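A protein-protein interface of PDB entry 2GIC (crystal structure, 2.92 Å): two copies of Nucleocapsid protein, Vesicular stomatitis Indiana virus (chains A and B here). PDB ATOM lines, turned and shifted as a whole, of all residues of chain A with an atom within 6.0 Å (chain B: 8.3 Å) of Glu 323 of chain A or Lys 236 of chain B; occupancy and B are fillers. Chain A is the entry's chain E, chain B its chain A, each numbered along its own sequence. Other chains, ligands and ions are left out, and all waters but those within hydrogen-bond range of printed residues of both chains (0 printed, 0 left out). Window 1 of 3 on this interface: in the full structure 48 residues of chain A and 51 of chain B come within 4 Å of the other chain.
ND1 of His 233 of chain B is in hydrogen-bond range of OD1 of Asp 321 of chain A (3.2 Å).
NH2 of Arg 252 of chain A is in hydrogen-bond range of O of Gly 239 of chain B (3.5 Å).
NH1 of Arg 312 of chain B is in salt-bridge range of OD1 of Asp 321 of chain A (3.0 Å).
N of Asp 343 of chain B is in hydrogen-bond range of OG of Ser 326 of chain A, 3.0 Å away.
OE1 of Glu 323 of chain A is in salt-bridge range of NH2 of Arg 373 of chain B.
NH2 of Arg 373 of chain B sits at hydrogen-bond distance from OG of Ser 326 of chain A (3.1 Å).
O of Thr 238 of chain B lies close to OE1 of Glu 323 of chain A (3.0 Å).
The side-chain carboxylate of Glu 323 of chain A lies close to the side-chain carboxylate of Asp 343 of chain B (2.9 Å).
NH1 of Arg 312 of chain B sits at hydrogen-bond distance from ND1 of His 233 of chain B (3.2 Å).
OG1 of Thr 238 of chain B sits at hydrogen-bond distance from O of Leu 234 of chain B.
O of Cys 235 of chain B lies within hydrogen-bond range of OG1 of Thr 238 of chain B, at 3.3 Å.
The backbone carbonyl oxygen of Thr 238 of chain B lies within hydrogen-bond range of the guanidinium group of Arg 373 of chain B, 2.9 Å away.
The side-chain carboxylate of Glu 253 of chain A lies within salt-bridge range of the guanidinium group of Arg 252 of chain A (3.0 Å).
OG1 of Thr 328 of chain A is in hydrogen-bond range of O of Thr 325 of chain A, 3.1 Å away.
Among the printed residues, pairs that only touch across the chains: Glu 323 of chain A with Gly 239 of chain B (3.2 Å), Asp 321 of chain A with Lys 236 of chain B (3.5 Å), Ser 326 of chain A with Ala 342 of chain B (3.5 Å), Tyr 324 of chain A with Ile 237 of chain B (3.5 Å), Ile 322 of chain A with Lys 236 of chain B (3.6 Å), Glu 323 of chain A with Ile 237 of chain B (3.6 Å), Glu 323 of chain A with Lys 236 of chain B (3.7 Å), Tyr 324 of chain A with Arg 309 of chain B (3.7 Å), Ile 322 of chain A with Ile 237 of chain B (3.8 Å), Ser 326 of chain A with Leu 344 of chain B (3.8 Å), Tyr 324 of chain A with Leu 308 of chain B (3.8 Å), Thr 325 of chain A with Val 338 of chain B (3.8 Å) and Thr 325 of chain A with Arg 309 of chain B (3.98 Å).
Printed residues of chain B within 4 Å of Asp 321 of chain A: His 233, Lys 236 and Arg 312.
Glu 323 of chain A touches just these residues of chain B: Lys 236 (3.7 Å), Ile 237 (3.6 Å), Thr 238 (3.0 Å), Gly 239 (3.2 Å), Asp 343 (2.9 Å) and Arg 373 (3.7 Å).
Lys 236 of chain B touches just these residues of chain A: Asp 321 (3.5 Å), Ile 322 (3.6 Å) and Glu 323 (3.7 Å).
Printed residues of chain A within 4 Å of Arg 312 of chain B: Asp 321.
Printed residues of chain A within 4 Å of Val 338 of chain B: Thr 325.
Of the printed residues of chain A, Arg 373 of chain B touches Glu 323 (3.7 Å) and Ser 326 (3.1 Å).
The nearest residue of chain B that does not touch Glu 323 of chain A is Val 338 of chain B (5.0 Å).
The nearest printed residue of chain A that does not touch Lys 236 of chain B is Tyr 324 of chain A (6.1 Å).
The nearest printed residue of chain A that does not touch Thr 238 of chain B is Ile 322 of chain A (5.6 Å).
Printed residues of chain B that touch a printed residue of chain A: His 233, Lys 236, Ile 237, Thr 238, Gly 239, Leu 308, Arg 309, Arg 312, Val 338, Ala 342, Asp 343, Leu 344 and Arg 373.
Hydrophobic or aromatic side chains of chain B that line the printed part of chain A: His 233, Ile 237 and Leu 344.
Printed residues of chain A that touch a printed residue of chain B: Arg 252, Asp 321, Ile 322, Glu 323, Tyr 324, Thr 325 and Ser 326.
Hydrophobic or aromatic side chains of chain A that line the printed part of chain B: Tyr 324.
No position is printed for both chains.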
ATOM      1  N   ASN A 251      -1.549  -5.046  -9.809  1.00  0.00           N
ATOM      2  CA  ASN A 251      -1.331  -5.393  -8.404  1.00  0.00           C
ATOM      3  C   ASN A 251      -1.094  -4.180  -7.501  1.00  0.00           C
ATOM      4  O   ASN A 251      -0.516  -3.172  -7.923  1.00  0.00           O
ATOM      5  CB  ASN A 251      -0.200  -6.407  -8.260  1.00  0.00           C
ATOM      6  CG  ASN A 251      -0.445  -7.657  -9.073  1.00  0.00           C
ATOM      7  OD1 ASN A 251      -0.426  -7.623 -10.308  1.00  0.00           O
ATOM      8  ND2 ASN A 251      -0.671  -8.774  -8.388  1.00  0.00           N
ATOM      9  N   ARG A 252      -1.557  -4.301  -6.260  1.00  0.00           N
ATOM     10  CA  ARG A 252      -1.420  -3.260  -5.248  1.00  0.00           C
ATOM     11  C   ARG A 252       0.058  -2.982  -4.899  1.00  0.00           C
ATOM     12  O   ARG A 252       0.459  -1.817  -4.757  1.00  0.00           O
ATOM     13  CB  ARG A 252      -2.246  -3.648  -4.010  1.00  0.00           C
ATOM     14  CG  ARG A 252      -1.909  -2.930  -2.698  1.00  0.00           C
ATOM     15  CD  ARG A 252      -2.758  -3.482  -1.542  1.00  0.00           C
ATOM     16  NE  ARG A 252      -2.800  -4.946  -1.556  1.00  0.00           N
ATOM     17  CZ  ARG A 252      -1.950  -5.733  -0.899  1.00  0.00           C
ATOM     18  NH1 ARG A 252      -0.989  -5.202  -0.147  1.00  0.00           N
ATOM     19  NH2 ARG A 252      -2.057  -7.057  -0.992  1.00  0.00           N
ATOM     20  N   GLU A 253       0.862  -4.037  -4.785  1.00  0.00           N
ATOM     21  CA  GLU A 253       2.266  -3.875  -4.405  1.00  0.00           C
ATOM     22  C   GLU A 253       3.104  -3.282  -5.533  1.00  0.00           C
ATOM     23  O   GLU A 253       4.145  -2.665  -5.295  1.00  0.00           O
ATOM     24  CB  GLU A 253       2.887  -5.176  -3.853  1.00  0.00           C
ATOM     25  CG  GLU A 253       2.167  -6.478  -4.210  1.00  0.00           C
ATOM     26  CD  GLU A 253       0.683  -6.486  -3.802  1.00  0.00           C
ATOM     27  OE1 GLU A 253      -0.173  -6.634  -4.711  1.00  0.00           O
ATOM     28  OE2 GLU A 253       0.367  -6.341  -2.592  1.00  0.00           O
ATOM     29  N   PHE A 299       9.745  -7.729 -11.257  1.00  0.00           N
ATOM     30  CA  PHE A 299       9.267  -9.021 -11.722  1.00  0.00           C
ATOM     31  C   PHE A 299       8.237  -8.815 -12.827  1.00  0.00           C
ATOM     32  O   PHE A 299       8.567  -8.871 -14.006  1.00  0.00           O
ATOM     33  CB  PHE A 299       8.672  -9.801 -10.548  1.00  0.00           C
ATOM     34  CG  PHE A 299       8.335 -11.231 -10.862  1.00  0.00           C
ATOM     35  CD1 PHE A 299       7.032 -11.600 -11.158  1.00  0.00           C
ATOM     36  CD2 PHE A 299       9.313 -12.213 -10.829  1.00  0.00           C
ATOM     37  CE1 PHE A 299       6.720 -12.926 -11.440  1.00  0.00           C
ATOM     38  CE2 PHE A 299       9.006 -13.538 -11.100  1.00  0.00           C
ATOM     39  CZ  PHE A 299       7.711 -13.895 -11.410  1.00  0.00           C
ATOM     40  N   ASP A 321      10.452 -13.315  -1.852  1.00  0.00           N
ATOM     41  CA  ASP A 321       9.433 -12.652  -1.031  1.00  0.00           C
ATOM     42  C   ASP A 321       8.424 -11.776  -1.783  1.00  0.00           C
ATOM     43  O   ASP A 321       8.095 -10.675  -1.327  1.00  0.00           O
ATOM     44  CB  ASP A 321      10.095 -11.831   0.083  1.00  0.00           C
ATOM     45  CG  ASP A 321      10.941 -12.678   1.017  1.00  0.00           C
ATOM     46  OD1 ASP A 321      10.363 -13.518   1.740  1.00  0.00           O
ATOM     47  OD2 ASP A 321      12.181 -12.484   1.046  1.00  0.00           O
ATOM     48  N   ILE A 322       7.938 -12.257  -2.926  1.00  0.00           N
ATOM     49  CA  ILE A 322       6.860 -11.577  -3.657  1.00  0.00           C
ATOM     50  C   ILE A 322       5.752 -12.551  -4.084  1.00  0.00           C
ATOM     51  O   ILE A 322       5.922 -13.774  -4.028  1.00  0.00           O
ATOM     52  CB  ILE A 322       7.379 -10.783  -4.897  1.00  0.00           C
ATOM     53  CG1 ILE A 322       8.137 -11.700  -5.866  1.00  0.00           C
ATOM     54  CG2 ILE A 322       8.228  -9.591  -4.460  1.00  0.00           C
ATOM     55  CD1 ILE A 322       8.419 -11.093  -7.228  1.00  0.00           C
ATOM     56  N   GLU A 323       4.624 -11.998  -4.511  1.00  0.00           N
ATOM     57  CA  GLU A 323       3.495 -12.797  -4.947  1.00  0.00           C
ATOM     58  C   GLU A 323       3.645 -13.263  -6.386  1.00  0.00           C
ATOM     59  O   GLU A 323       3.095 -12.633  -7.303  1.00  0.00           O
ATOM     60  CB  GLU A 323       2.229 -11.974  -4.851  1.00  0.00           C
ATOM     61  CG  GLU A 323       1.657 -11.865  -3.491  1.00  0.00           C
ATOM     62  CD  GLU A 323       0.223 -11.433  -3.562  1.00  0.00           C
ATOM     63  OE1 GLU A 323      -0.649 -12.264  -3.919  1.00  0.00           O
ATOM     64  OE2 GLU A 323      -0.030 -10.241  -3.283  1.00  0.00           O
ATOM     65  N   TYR A 324       4.357 -14.367  -6.600  1.00  0.00           N
ATOM     66  CA  TYR A 324       4.567 -14.853  -7.962  1.00  0.00           C
ATOM     67  C   TYR A 324       3.271 -15.149  -8.711  1.00  0.00           C
ATOM     68  O   TYR A 324       3.099 -14.679  -9.834  1.00  0.00           O
ATOM     69  CB  TYR A 324       5.500 -16.063  -7.993  1.00  0.00           C
ATOM     70  CG  TYR A 324       6.803 -15.815  -7.280  1.00  0.00           C
ATOM     71  CD1 TYR A 324       7.050 -16.399  -6.047  1.00  0.00           C
ATOM     72  CD2 TYR A 324       7.779 -14.979  -7.828  1.00  0.00           C
ATOM     73  CE1 TYR A 324       8.224 -16.167  -5.381  1.00  0.00           C
ATOM     74  CE2 TYR A 324       8.964 -14.750  -7.171  1.00  0.00           C
ATOM     75  CZ  TYR A 324       9.176 -15.345  -5.944  1.00  0.00           C
ATOM     76  OH  TYR A 324      10.342 -15.132  -5.261  1.00  0.00           O
ATOM     77  N   THR A 325       2.353 -15.893  -8.095  1.00  0.00           N
ATOM     78  CA  THR A 325       1.151 -16.327  -8.811  1.00  0.00           C
ATOM     79  C   THR A 325       0.385 -15.139  -9.398  1.00  0.00           C
ATOM     80  O   THR A 325       0.213 -15.057 -10.616  1.00  0.00           O
ATOM     81  CB  THR A 325       0.195 -17.207  -7.963  1.00  0.00           C
ATOM     82  OG1 THR A 325      -0.524 -16.394  -7.019  1.00  0.00           O
ATOM     83  CG2 THR A 325       0.942 -18.341  -7.271  1.00  0.00           C
ATOM     84  N   SER A 326      -0.042 -14.224  -8.528  1.00  0.00           N
ATOM     85  CA  SER A 326      -0.777 -13.019  -8.924  1.00  0.00           C
ATOM     86  C   SER A 326      -0.013 -12.158  -9.931  1.00  0.00           C
ATOM     87  O   SER A 326      -0.562 -11.756 -10.960  1.00  0.00           O
ATOM     88  CB  SER A 326      -1.154 -12.197  -7.695  1.00  0.00           C
ATOM     89  OG  SER A 326      -2.371 -12.661  -7.138  1.00  0.00           O
ATOM     90  N   LEU A 327       1.257 -11.895  -9.638  1.00  0.00           N
ATOM     91  CA  LEU A 327       2.110 -11.114 -10.533  1.00  0.00           C
ATOM     92  C   LEU A 327       2.220 -11.733 -11.927  1.00  0.00           C
ATOM     93  O   LEU A 327       2.189 -11.020 -12.921  1.00  0.00           O
ATOM     94  CB  LEU A 327       3.498 -10.902  -9.912  1.00  0.00           C
ATOM     95  CG  LEU A 327       3.807  -9.632  -9.097  1.00  0.00           C
ATOM     96  CD1 LEU A 327       2.596  -8.977  -8.470  1.00  0.00           C
ATOM     97  CD2 LEU A 327       4.842  -9.923  -8.021  1.00  0.00           C
ATOM     98  N   THR A 328       2.326 -13.058 -12.003  1.00  0.00           N
ATOM     99  CA  THR A 328       2.485 -13.701 -13.308  1.00  0.00           C
ATOM    100  C   THR A 328       1.174 -13.765 -14.098  1.00  0.00           C
ATOM    101  O   THR A 328       1.146 -13.454 -15.297  1.00  0.00           O
ATOM    102  CB  THR A 328       3.138 -15.091 -13.232  1.00  0.00           C
ATOM    103  OG1 THR A 328       2.184 -16.051 -12.781  1.00  0.00           O
ATOM    104  CG2 THR A 328       4.323 -15.068 -12.298  1.00  0.00           C
ATOM    105  N   ALA B 229      10.462 -16.841  10.695  1.00  0.00           N
ATOM    106  CA  ALA B 229      10.799 -16.380   9.354  1.00  0.00           C
ATOM    107  C   ALA B 229       9.916 -17.020   8.292  1.00  0.00           C
ATOM    108  O   ALA B 229       9.614 -16.386   7.286  1.00  0.00           O
ATOM    109  CB  ALA B 229      12.270 -16.609   9.053  1.00  0.00           C
ATOM    110  N   THR B 230       9.485 -18.260   8.502  1.00  0.00           N
ATOM    111  CA  THR B 230       8.598 -18.876   7.517  1.00  0.00           C
ATOM    112  C   THR B 230       7.237 -18.191   7.521  1.00  0.00           C
ATOM    113  O   THR B 230       6.640 -17.997   6.472  1.00  0.00           O
ATOM    114  CB  THR B 230       8.510 -20.433   7.609  1.00  0.00           C
ATOM    115  OG1 THR B 230       7.141 -20.861   7.546  1.00  0.00           O
ATOM    116  CG2 THR B 230       9.137 -20.948   8.879  1.00  0.00           C
ATOM    117  N   PHE B 231       6.780 -17.797   8.707  1.00  0.00           N
ATOM    118  CA  PHE B 231       5.536 -17.037   8.852  1.00  0.00           C
ATOM    119  C   PHE B 231       5.626 -15.678   8.137  1.00  0.00           C
ATOM    120  O   PHE B 231       4.653 -15.226   7.517  1.00  0.00           O
ATOM    121  CB  PHE B 231       5.165 -16.883  10.333  1.00  0.00           C
ATOM    122  CG  PHE B 231       3.916 -16.080  10.577  1.00  0.00           C
ATOM    123  CD1 PHE B 231       2.731 -16.367   9.893  1.00  0.00           C
ATOM    124  CD2 PHE B 231       3.915 -15.044  11.512  1.00  0.00           C
ATOM    125  CE1 PHE B 231       1.578 -15.622  10.117  1.00  0.00           C
ATOM    126  CE2 PHE B 231       2.768 -14.305  11.751  1.00  0.00           C
ATOM    127  CZ  PHE B 231       1.596 -14.592  11.049  1.00  0.00           C
ATOM    128  N   GLY B 232       6.801 -15.051   8.207  1.00  0.00           N
ATOM    129  CA  GLY B 232       7.089 -13.845   7.437  1.00  0.00           C
ATOM    130  C   GLY B 232       7.004 -14.161   5.962  1.00  0.00           C
ATOM    131  O   GLY B 232       6.128 -13.659   5.258  1.00  0.00           O
ATOM    132  N   HIS B 233       7.894 -15.038   5.511  1.00  0.00           N
ATOM    133  CA  HIS B 233       7.964 -15.468   4.117  1.00  0.00           C
ATOM    134  C   HIS B 233       6.614 -15.890   3.515  1.00  0.00           C
ATOM    135  O   HIS B 233       6.348 -15.647   2.338  1.00  0.00           O
ATOM    136  CB  HIS B 233       8.984 -16.599   3.980  1.00  0.00           C
ATOM    137  CG  HIS B 233       9.006 -17.224   2.622  1.00  0.00           C
ATOM    138  ND1 HIS B 233       9.488 -16.566   1.508  1.00  0.00           N
ATOM    139  CD2 HIS B 233       8.587 -18.438   2.190  1.00  0.00           C
ATOM    140  CE1 HIS B 233       9.367 -17.348   0.449  1.00  0.00           C
ATOM    141  NE2 HIS B 233       8.829 -18.492   0.836  1.00  0.00           N
ATOM    142  N   LEU B 234       5.771 -16.526   4.325  1.00  0.00           N
ATOM    143  CA  LEU B 234       4.485 -17.020   3.862  1.00  0.00           C
ATOM    144  C   LEU B 234       3.549 -15.865   3.526  1.00  0.00           C
ATOM    145  O   LEU B 234       2.855 -15.906   2.504  1.00  0.00           O
ATOM    146  CB  LEU B 234       3.856 -17.964   4.893  1.00  0.00           C
ATOM    147  CG  LEU B 234       2.515 -18.644   4.568  1.00  0.00           C
ATOM    148  CD1 LEU B 234       2.607 -19.561   3.340  1.00  0.00           C
ATOM    149  CD2 LEU B 234       1.992 -19.413   5.784  1.00  0.00           C
ATOM    150  N   CYS B 235       3.543 -14.838   4.382  1.00  0.00           N
ATOM    151  CA  CYS B 235       2.770 -13.617   4.137  1.00  0.00           C
ATOM    152  C   CYS B 235       3.159 -12.956   2.827  1.00  0.00           C
ATOM    153  O   CYS B 235       2.293 -12.632   2.019  1.00  0.00           O
ATOM    154  CB  CYS B 235       2.949 -12.618   5.274  1.00  0.00           C
ATOM    155  SG  CYS B 235       2.170 -13.135   6.793  1.00  0.00           S
ATOM    156  N   LYS B 236       4.463 -12.767   2.628  1.00  0.00           N
ATOM    157  CA  LYS B 236       4.990 -12.191   1.395  1.00  0.00           C
ATOM    158  C   LYS B 236       4.601 -13.009   0.168  1.00  0.00           C
ATOM    159  O   LYS B 236       4.170 -12.431  -0.826  1.00  0.00           O
ATOM    160  CB  LYS B 236       6.516 -12.039   1.458  1.00  0.00           C
ATOM    161  CG  LYS B 236       7.031 -11.097   2.545  1.00  0.00           C
ATOM    162  CD  LYS B 236       7.069  -9.645   2.085  1.00  0.00           C
ATOM    163  CE  LYS B 236       7.577  -8.743   3.203  1.00  0.00           C
ATOM    164  NZ  LYS B 236       7.771  -7.329   2.775  1.00  0.00           N
ATOM    165  N   ILE B 237       4.748 -14.337   0.245  1.00  0.00           N
ATOM    166  CA  ILE B 237       4.431 -15.240  -0.876  1.00  0.00           C
ATOM    167  C   ILE B 237       2.957 -15.219  -1.256  1.00  0.00           C
ATOM    168  O   ILE B 237       2.632 -15.264  -2.436  1.00  0.00           O
ATOM    169  CB  ILE B 237       4.937 -16.708  -0.622  1.00  0.00           C
ATOM    170  CG1 ILE B 237       6.259 -16.959  -1.346  1.00  0.00           C
ATOM    171  CG2 ILE B 237       3.941 -17.779  -1.085  1.00  0.00           C
ATOM    172  CD1 ILE B 237       6.102 -17.413  -2.790  1.00  0.00           C
ATOM    173  N   THR B 238       2.075 -15.144  -0.262  1.00  0.00           N
ATOM    174  CA  THR B 238       0.629 -15.143  -0.506  1.00  0.00           C
ATOM    175  C   THR B 238       0.084 -13.734  -0.725  1.00  0.00           C
ATOM    176  O   THR B 238      -1.024 -13.556  -1.228  1.00  0.00           O
ATOM    177  CB  THR B 238      -0.153 -15.767   0.669  1.00  0.00           C
ATOM    178  OG1 THR B 238       0.042 -14.972   1.847  1.00  0.00           O
ATOM    179  CG2 THR B 238       0.299 -17.197   0.927  1.00  0.00           C
ATOM    180  N   GLY B 239       0.865 -12.741  -0.321  1.00  0.00           N
ATOM    181  CA  GLY B 239       0.407 -11.364  -0.293  1.00  0.00           C
ATOM    182  C   GLY B 239      -0.750 -11.130   0.658  1.00  0.00           C
ATOM    183  O   GLY B 239      -1.397 -10.092   0.599  1.00  0.00           O
ATOM    184  N   MET B 240      -1.009 -12.092   1.536  1.00  0.00           N
ATOM    185  CA  MET B 240      -2.113 -11.987   2.480  1.00  0.00           C
ATOM    186  C   MET B 240      -1.721 -11.232   3.745  1.00  0.00           C
ATOM    187  O   MET B 240      -0.537 -11.043   4.044  1.00  0.00           O
ATOM    188  CB  MET B 240      -2.684 -13.368   2.821  1.00  0.00           C
ATOM    189  CG  MET B 240      -3.469 -13.997   1.676  1.00  0.00           C
ATOM    190  SD  MET B 240      -4.427 -15.451   2.137  1.00  0.00           S
ATOM    191  CE  MET B 240      -5.867 -14.717   2.902  1.00  0.00           C
ATOM    192  N   SER B 241      -2.743 -10.789   4.470  1.00  0.00           N
ATOM    193  CA  SER B 241      -2.578 -10.107   5.738  1.00  0.00           C
ATOM    194  C   SER B 241      -1.975 -11.041   6.766  1.00  0.00           C
ATOM    195  O   SER B 241      -2.084 -12.261   6.644  1.00  0.00           O
ATOM    196  CB  SER B 241      -3.933  -9.635   6.235  1.00  0.00           C
ATOM    197  OG  SER B 241      -3.861  -9.306   7.605  1.00  0.00           O
ATOM    198  N   THR B 242      -1.343 -10.473   7.789  1.00  0.00           N
ATOM    199  CA  THR B 242      -0.776 -11.297   8.849  1.00  0.00           C
ATOM    200  C   THR B 242      -1.878 -12.033   9.626  1.00  0.00           C
ATOM    201  O   THR B 242      -1.686 -13.170  10.062  1.00  0.00           O
ATOM    202  CB  THR B 242       0.158 -10.494   9.781  1.00  0.00           C
ATOM    203  OG1 THR B 242       1.145 -11.374  10.324  1.00  0.00           O
ATOM    204  CG2 THR B 242      -0.609  -9.811  10.928  1.00  0.00           C
ATOM    205  N   VAL B 245      -3.522 -14.864   6.942  1.00  0.00           N
ATOM    206  CA  VAL B 245      -2.726 -16.074   6.887  1.00  0.00           C
ATOM    207  C   VAL B 245      -3.124 -16.927   8.083  1.00  0.00           C
ATOM    208  O   VAL B 245      -3.311 -18.140   7.948  1.00  0.00           O
ATOM    209  CB  VAL B 245      -1.221 -15.739   6.930  1.00  0.00           C
ATOM    210  CG1 VAL B 245      -0.403 -16.981   7.162  1.00  0.00           C
ATOM    211  CG2 VAL B 245      -0.795 -15.052   5.652  1.00  0.00           C
ATOM    212  N   LEU B 308       3.301 -22.418  -4.108  1.00  0.00           N
ATOM    213  CA  LEU B 308       3.187 -21.034  -4.570  1.00  0.00           C
ATOM    214  C   LEU B 308       4.478 -20.479  -5.174  1.00  0.00           C
ATOM    215  O   LEU B 308       4.720 -19.277  -5.115  1.00  0.00           O
ATOM    216  CB  LEU B 308       2.692 -20.134  -3.442  1.00  0.00           C
ATOM    217  CG  LEU B 308       1.205 -19.792  -3.321  1.00  0.00           C
ATOM    218  CD1 LEU B 308       0.287 -20.854  -3.928  1.00  0.00           C
ATOM    219  CD2 LEU B 308       0.853 -19.531  -1.861  1.00  0.00           C
ATOM    220  N   ARG B 309       5.286 -21.367  -5.758  1.00  0.00           N
ATOM    221  CA  ARG B 309       6.467 -21.021  -6.573  1.00  0.00           C
ATOM    222  C   ARG B 309       7.671 -20.450  -5.800  1.00  0.00           C
ATOM    223  O   ARG B 309       8.551 -19.814  -6.392  1.00  0.00           O
ATOM    224  CB  ARG B 309       6.080 -20.115  -7.760  1.00  0.00           C
ATOM    225  CG  ARG B 309       5.252 -20.816  -8.848  1.00  0.00           C
ATOM    226  CD  ARG B 309       3.760 -20.878  -8.490  1.00  0.00           C
ATOM    227  NE  ARG B 309       3.181 -22.200  -8.735  1.00  0.00           N
ATOM    228  CZ  ARG B 309       2.551 -22.559  -9.852  1.00  0.00           C
ATOM    229  NH1 ARG B 309       2.396 -21.696 -10.850  1.00  0.00           N
ATOM    230  NH2 ARG B 309       2.064 -23.791  -9.966  1.00  0.00           N
ATOM    231  N   ARG B 312      13.052 -20.811  -2.091  1.00  0.00           N
ATOM    232  CA  ARG B 312      13.731 -21.190  -0.851  1.00  0.00           C
ATOM    233  C   ARG B 312      13.183 -22.510  -0.307  1.00  0.00           C
ATOM    234  O   ARG B 312      13.955 -23.389   0.088  1.00  0.00           O
ATOM    235  CB  ARG B 312      13.691 -20.073   0.196  1.00  0.00           C
ATOM    236  CG  ARG B 312      12.339 -19.409   0.360  1.00  0.00           C
ATOM    237  CD  ARG B 312      12.391 -18.226   1.324  1.00  0.00           C
ATOM    238  NE  ARG B 312      13.241 -17.132   0.843  1.00  0.00           N
ATOM    239  CZ  ARG B 312      13.242 -15.896   1.344  1.00  0.00           C
ATOM    240  NH1 ARG B 312      12.421 -15.567   2.351  1.00  0.00           N
ATOM    241  NH2 ARG B 312      14.069 -14.986   0.834  1.00  0.00           N
ATOM    242  N   VAL B 338      -5.087 -19.414  -3.128  1.00  0.00           N
ATOM    243  CA  VAL B 338      -4.308 -18.247  -3.547  1.00  0.00           C
ATOM    244  C   VAL B 338      -4.007 -18.247  -5.057  1.00  0.00           C
ATOM    245  O   VAL B 338      -4.049 -17.196  -5.707  1.00  0.00           O
ATOM    246  CB  VAL B 338      -2.979 -18.184  -2.754  1.00  0.00           C
ATOM    247  CG1 VAL B 338      -2.147 -16.978  -3.157  1.00  0.00           C
ATOM    248  CG2 VAL B 338      -3.261 -18.162  -1.267  1.00  0.00           C
ATOM    249  N   GLY B 339      -3.701 -19.423  -5.604  1.00  0.00           N
ATOM    250  CA  GLY B 339      -3.290 -19.537  -6.995  1.00  0.00           C
ATOM    251  C   GLY B 339      -4.475 -19.541  -7.928  1.00  0.00           C
ATOM    252  O   GLY B 339      -4.353 -19.212  -9.107  1.00  0.00           O
ATOM    253  N   SER B 341      -7.062 -17.762  -7.262  1.00  0.00           N
ATOM    254  CA  SER B 341      -7.621 -16.428  -7.101  1.00  0.00           C
ATOM    255  C   SER B 341      -6.529 -15.374  -7.146  1.00  0.00           C
ATOM    256  O   SER B 341      -5.896 -15.080  -6.133  1.00  0.00           O
ATOM    257  CB  SER B 341      -8.388 -16.328  -5.785  1.00  0.00           C
ATOM    258  OG  SER B 341      -9.310 -17.393  -5.665  1.00  0.00           O
ATOM    259  N   ALA B 342      -6.305 -14.817  -8.331  1.00  0.00           N
ATOM    260  CA  ALA B 342      -5.424 -13.665  -8.488  1.00  0.00           C
ATOM    261  C   ALA B 342      -6.005 -12.449  -7.778  1.00  0.00           C
ATOM    262  O   ALA B 342      -7.230 -12.326  -7.631  1.00  0.00           O
ATOM    263  CB  ALA B 342      -5.221 -13.354  -9.954  1.00  0.00           C
ATOM    264  N   ASP B 343      -5.122 -11.560  -7.331  1.00  0.00           N
ATOM    265  CA  ASP B 343      -5.544 -10.287  -6.747  1.00  0.00           C
ATOM    266  C   ASP B 343      -6.234  -9.433  -7.807  1.00  0.00           C
ATOM    267  O   ASP B 343      -7.455  -9.297  -7.795  1.00  0.00           O
ATOM    268  CB  ASP B 343      -4.352  -9.557  -6.126  1.00  0.00           C
ATOM    269  CG  ASP B 343      -3.871 -10.219  -4.850  1.00  0.00           C
ATOM    270  OD1 ASP B 343      -2.642 -10.377  -4.691  1.00  0.00           O
ATOM    271  OD2 ASP B 343      -4.722 -10.586  -4.007  1.00  0.00           O
ATOM    272  N   LEU B 344      -5.443  -8.875  -8.718  1.00  0.00           N
ATOM    273  CA  LEU B 344      -5.946  -8.251  -9.941  1.00  0.00           C
ATOM    274  C   LEU B 344      -7.062  -7.221  -9.755  1.00  0.00           C
ATOM    275  O   LEU B 344      -8.242  -7.560  -9.660  1.00  0.00           O
ATOM    276  CB  LEU B 344      -6.352  -9.332 -10.951  1.00  0.00           C
ATOM    277  CG  LEU B 344      -5.274  -9.888 -11.890  1.00  0.00           C
ATOM    278  CD1 LEU B 344      -5.279  -9.120 -13.199  1.00  0.00           C
ATOM    279  CD2 LEU B 344      -3.860  -9.911 -11.274  1.00  0.00           C
ATOM    280  N   ARG B 373     -10.670 -15.305  -1.465  1.00  0.00           N
ATOM    281  CA  ARG B 373      -9.673 -16.091  -0.751  1.00  0.00           C
ATOM    282  C   ARG B 373     -10.073 -16.342   0.704  1.00  0.00           C
ATOM    283  O   ARG B 373      -9.234 -16.665   1.542  1.00  0.00           O
ATOM    284  CB  ARG B 373      -8.314 -15.396  -0.807  1.00  0.00           C
ATOM    285  CG  ARG B 373      -7.707 -15.274  -2.192  1.00  0.00           C
ATOM    286  CD  ARG B 373      -6.249 -14.908  -2.068  1.00  0.00           C
ATOM    287  NE  ARG B 373      -5.680 -14.432  -3.321  1.00  0.00           N
ATOM    288  CZ  ARG B 373      -4.409 -14.075  -3.476  1.00  0.00           C
ATOM    289  NH1 ARG B 373      -3.563 -14.141  -2.460  1.00  0.00           N
ATOM    290  NH2 ARG B 373      -3.977 -13.649  -4.651  1.00  0.00           N
